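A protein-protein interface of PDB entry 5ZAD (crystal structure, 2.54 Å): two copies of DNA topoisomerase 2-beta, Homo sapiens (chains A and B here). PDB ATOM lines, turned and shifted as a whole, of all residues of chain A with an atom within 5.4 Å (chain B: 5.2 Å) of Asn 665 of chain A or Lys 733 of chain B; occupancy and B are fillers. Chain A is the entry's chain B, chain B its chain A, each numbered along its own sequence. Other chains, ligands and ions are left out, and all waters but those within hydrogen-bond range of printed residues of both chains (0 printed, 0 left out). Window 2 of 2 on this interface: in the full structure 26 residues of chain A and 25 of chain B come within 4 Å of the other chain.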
ATOM      1  N   ILE A 663     -22.257   6.080   0.933  1.00  0.00           N
ATOM      2  CA  ILE A 663     -23.392   5.482   1.615  1.00  0.00           C
ATOM      3  C   ILE A 663     -23.229   3.978   1.822  1.00  0.00           C
ATOM      4  O   ILE A 663     -23.896   3.412   2.704  1.00  0.00           O
ATOM      5  CB  ILE A 663     -24.697   5.814   0.857  1.00  0.00           C
ATOM      6  CG1 ILE A 663     -24.701   5.201  -0.544  1.00  0.00           C
ATOM      7  CG2 ILE A 663     -24.840   7.319   0.705  1.00  0.00           C
ATOM      8  CD1 ILE A 663     -25.306   3.859  -0.643  1.00  0.00           C
ATOM      9  N   GLU A 664     -22.332   3.323   1.084  1.00  0.00           N
ATOM     10  CA  GLU A 664     -22.057   1.901   1.258  1.00  0.00           C
ATOM     11  C   GLU A 664     -21.751   1.558   2.710  1.00  0.00           C
ATOM     12  O   GLU A 664     -20.864   2.152   3.328  1.00  0.00           O
ATOM     13  CB  GLU A 664     -20.888   1.497   0.360  1.00  0.00           C
ATOM     14  CG  GLU A 664     -21.269   1.276  -1.093  1.00  0.00           C
ATOM     15  CD  GLU A 664     -21.342   2.550  -1.919  1.00  0.00           C
ATOM     16  OE1 GLU A 664     -21.488   3.653  -1.347  1.00  0.00           O
ATOM     17  OE2 GLU A 664     -21.261   2.431  -3.158  1.00  0.00           O
ATOM     18  N   ASN A 665     -22.486   0.575   3.228  1.00  0.00           N
ATOM     19  CA  ASN A 665     -22.412   0.090   4.611  1.00  0.00           C
ATOM     20  C   ASN A 665     -22.167   1.229   5.578  1.00  0.00           C
ATOM     21  O   ASN A 665     -21.163   1.282   6.287  1.00  0.00           O
ATOM     22  CB  ASN A 665     -21.349  -0.980   4.822  1.00  0.00           C
ATOM     23  CG  ASN A 665     -21.600  -1.802   6.073  1.00  0.00           C
ATOM     24  OD1 ASN A 665     -20.987  -2.846   6.273  1.00  0.00           O
ATOM     25  ND2 ASN A 665     -22.533  -1.348   6.910  1.00  0.00           N
ATOM     26  N   ARG A 666     -23.117   2.145   5.600  1.00  0.00           N
ATOM     27  CA  ARG A 666     -23.150   3.108   6.661  1.00  0.00           C
ATOM     28  C   ARG A 666     -24.405   2.783   7.454  1.00  0.00           C
ATOM     29  O   ARG A 666     -24.900   1.648   7.404  1.00  0.00           O
ATOM     30  CB  ARG A 666     -23.105   4.521   6.083  1.00  0.00           C
ATOM     31  CG  ARG A 666     -22.063   4.654   4.986  1.00  0.00           C
ATOM     32  CD  ARG A 666     -20.693   5.021   5.528  1.00  0.00           C
ATOM     33  NE  ARG A 666     -20.757   6.151   6.450  1.00  0.00           N
ATOM     34  CZ  ARG A 666     -20.893   7.418   6.070  1.00  0.00           C
ATOM     35  NH1 ARG A 666     -20.936   8.383   6.979  1.00  0.00           N
ATOM     36  NH2 ARG A 666     -21.009   7.723   4.786  1.00  0.00           N
ATOM     37  N   SER A 667     -24.935   3.762   8.170  1.00  0.00           N
ATOM     38  CA  SER A 667     -26.074   3.465   9.011  1.00  0.00           C
ATOM     39  C   SER A 667     -27.075   4.598   8.958  1.00  0.00           C
ATOM     40  O   SER A 667     -26.752   5.748   8.630  1.00  0.00           O
ATOM     41  CB  SER A 667     -25.696   3.182  10.463  1.00  0.00           C
ATOM     42  OG  SER A 667     -26.871   2.825  11.174  1.00  0.00           O
ATOM     43  N   ILE B 657     -20.401  -3.212  -1.706  1.00  0.00           N
ATOM     44  CA  ILE B 657     -20.133  -2.886  -0.326  1.00  0.00           C
ATOM     45  C   ILE B 657     -18.658  -2.626  -0.068  1.00  0.00           C
ATOM     46  O   ILE B 657     -18.320  -1.524   0.361  1.00  0.00           O
ATOM     47  CB  ILE B 657     -20.801  -3.993   0.523  1.00  0.00           C
ATOM     48  CG1 ILE B 657     -22.242  -3.662   0.668  1.00  0.00           C
ATOM     49  CG2 ILE B 657     -19.997  -4.471   1.767  1.00  0.00           C
ATOM     50  CD1 ILE B 657     -22.354  -2.397   1.479  1.00  0.00           C
ATOM     51  N   LEU B 731     -27.687  -0.638   0.172  1.00  0.00           N
ATOM     52  CA  LEU B 731     -26.299  -0.482   0.626  1.00  0.00           C
ATOM     53  C   LEU B 731     -26.295   0.082   2.047  1.00  0.00           C
ATOM     54  O   LEU B 731     -26.011   1.265   2.242  1.00  0.00           O
ATOM     55  CB  LEU B 731     -25.579   0.431  -0.355  1.00  0.00           C
ATOM     56  CG  LEU B 731     -26.018   0.308  -1.825  1.00  0.00           C
ATOM     57  CD1 LEU B 731     -25.166   1.172  -2.725  1.00  0.00           C
ATOM     58  CD2 LEU B 731     -25.944  -1.143  -2.326  1.00  0.00           C
ATOM     59  N   THR B 732     -26.612  -0.744   3.048  1.00  0.00           N
ATOM     60  CA  THR B 732     -26.843  -0.152   4.366  1.00  0.00           C
ATOM     61  C   THR B 732     -26.680  -1.217   5.441  1.00  0.00           C
ATOM     62  O   THR B 732     -26.934  -2.395   5.194  1.00  0.00           O
ATOM     63  CB  THR B 732     -28.246   0.503   4.436  1.00  0.00           C
ATOM     64  OG1 THR B 732     -28.246   1.726   3.695  1.00  0.00           O
ATOM     65  CG2 THR B 732     -28.703   0.811   5.863  1.00  0.00           C
ATOM     66  N   LYS B 733     -26.244  -0.776   6.629  1.00  0.00           N
ATOM     67  CA  LYS B 733     -25.975  -1.669   7.752  1.00  0.00           C
ATOM     68  C   LYS B 733     -27.158  -2.593   8.027  1.00  0.00           C
ATOM     69  O   LYS B 733     -26.983  -3.793   8.271  1.00  0.00           O
ATOM     70  CB  LYS B 733     -25.650  -0.803   8.988  1.00  0.00           C
ATOM     71  CG  LYS B 733     -25.733  -1.435  10.389  1.00  0.00           C
ATOM     72  CD  LYS B 733     -24.936  -2.716  10.557  1.00  0.00           C
ATOM     73  CE  LYS B 733     -25.459  -3.534  11.742  1.00  0.00           C
ATOM     74  NZ  LYS B 733     -26.239  -4.736  11.303  1.00  0.00           N
ATOM     75  N   GLU B 734     -28.373  -2.050   7.973  1.00  0.00           N
ATOM     76  CA  GLU B 734     -29.584  -2.820   8.208  1.00  0.00           C
ATOM     77  C   GLU B 734     -30.288  -3.285   6.939  1.00  0.00           C
ATOM     78  O   GLU B 734     -31.409  -3.797   7.025  1.00  0.00           O
ATOM     79  CB  GLU B 734     -30.543  -2.017   9.078  1.00  0.00           C
ATOM     80  CG  GLU B 734     -29.875  -1.507  10.322  1.00  0.00           C
ATOM     81  CD  GLU B 734     -29.143  -0.209  10.088  1.00  0.00           C
ATOM     82  OE1 GLU B 734     -28.964   0.540  11.058  1.00  0.00           O
ATOM     83  OE2 GLU B 734     -28.751   0.069   8.935  1.00  0.00           O
ATOM     84  N   LYS B 735     -29.645  -3.193   5.776  1.00  0.00           N
ATOM     85  CA  LYS B 735     -30.172  -3.836   4.582  1.00  0.00           C
ATOM     86  C   LYS B 735     -29.310  -4.992   4.121  1.00  0.00           C
ATOM     87  O   LYS B 735     -29.798  -5.851   3.379  1.00  0.00           O
ATOM     88  CB  LYS B 735     -30.337  -2.840   3.426  1.00  0.00           C
ATOM     89  CG  LYS B 735     -31.061  -1.533   3.775  1.00  0.00           C
ATOM     90  CD  LYS B 735     -32.205  -1.705   4.765  1.00  0.00           C
ATOM     91  CE  LYS B 735     -33.472  -2.248   4.123  1.00  0.00           C
ATOM     92  NZ  LYS B 735     -34.675  -1.529   4.625  1.00  0.00           N
ATOM     93  N   VAL B 736     -28.045  -5.021   4.524  1.00  0.00           N
ATOM     94  CA  VAL B 736     -27.199  -6.157   4.202  1.00  0.00           C
ATOM     95  C   VAL B 736     -27.539  -7.344   5.101  1.00  0.00           C
ATOM     96  O   VAL B 736     -27.904  -8.419   4.611  1.00  0.00           O
ATOM     97  CB  VAL B 736     -25.718  -5.748   4.299  1.00  0.00           C
ATOM     98  CG1 VAL B 736     -25.384  -4.795   3.170  1.00  0.00           C
ATOM     99  CG2 VAL B 736     -25.424  -5.072   5.635  1.00  0.00           C
ATOM    100  N   GLU B 737     -27.506  -7.147   6.430  1.00  0.00           N
ATOM    101  CA  GLU B 737     -27.883  -8.233   7.334  1.00  0.00           C
ATOM    102  C   GLU B 737     -29.346  -8.610   7.158  1.00  0.00           C
ATOM    103  O   GLU B 737     -29.736  -9.741   7.458  1.00  0.00           O
ATOM    104  CB  GLU B 737     -27.579  -7.857   8.803  1.00  0.00           C
ATOM    105  CG  GLU B 737     -28.758  -7.372   9.668  1.00  0.00           C
ATOM    106  CD  GLU B 737     -29.522  -6.232   9.037  1.00  0.00           C
ATOM    107  OE1 GLU B 737     -28.936  -5.589   8.151  1.00  0.00           O
ATOM    108  OE2 GLU B 737     -30.699  -6.002   9.391  1.00  0.00           O
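No position is printed for both chains. Of the 8 pairs that touch across the chains among the printed residues, none has its exchanged pair printed and touching as well.
Of the 8 printed residues of chain B, 5 touch a printed residue of chain A. Printed residues of chain B that touch a printed residue of chain A: Ile 657, Leu 731, Thr 732, Lys 733 and Glu 734.
Asn 665 of chain A touches just these residues of chain B: Ile 657 (3.5 Å), Leu 731 (3.7 Å) and Lys 733 (3.6 Å). Of chain A, only Asn 665 (3.6 Å) and Arg 666 (2.9 Å) come within 4 Å of Lys 733 of chain B. Printed residues of chain B within 4 Å of Glu 664 of chain A: Ile 657 (3.96 Å). Of the printed residues of chain A, Thr 732 of chain B touches Arg 666. Of the printed residues of chain A, Ile 657 of chain B touches Glu 664 (3.96 Å) and Asn 665 (3.5 Å). Of the printed residues of chain B, Ser 667 of chain A touches Glu 734. Lys 735 of chain B touches none of the printed residues of chain A. The nearest residue of chain A that does not touch Lys 733 of chain B is Ser 667 of chain A (4.2 Å).
Glu 664 of chain A touches Ile 657 of chain B (CB to O, 3.96 Å). Ile 657 of chain B touches Asn 665 of chain A (CD1 to N, 3.5 Å). Asn 665 of chain A touches Leu 731 of chain B (N to O, 3.7 Å). Lys 733 of chain B touches Asn 665 of chain A (CA to ND2, 3.6 Å). O of Arg 666 of chain A touches C of Thr 732 of chain B, 3.9 Å away.
The backbone carbonyl oxygen (O) of Arg 666 of chain A is in hydrogen-bond range of the backbone NH (N) of Lys 733 of chain B (2.9 Å). OE1 of Glu 734 of chain B lies within hydrogen-bond range of OG of Ser 667 of chain A (3.1 Å). The backbone carbonyl oxygen (O) of Leu 731 of chain B lies close to the backbone carbonyl oxygen (O) of Ile 663 of chain A (3.0 Å).
The side-chain carboxylate (OE1) of Glu 737 of chain B lies close to the backbone carbonyl oxygen (O) of Lys 733 of chain B (2.7 Å).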
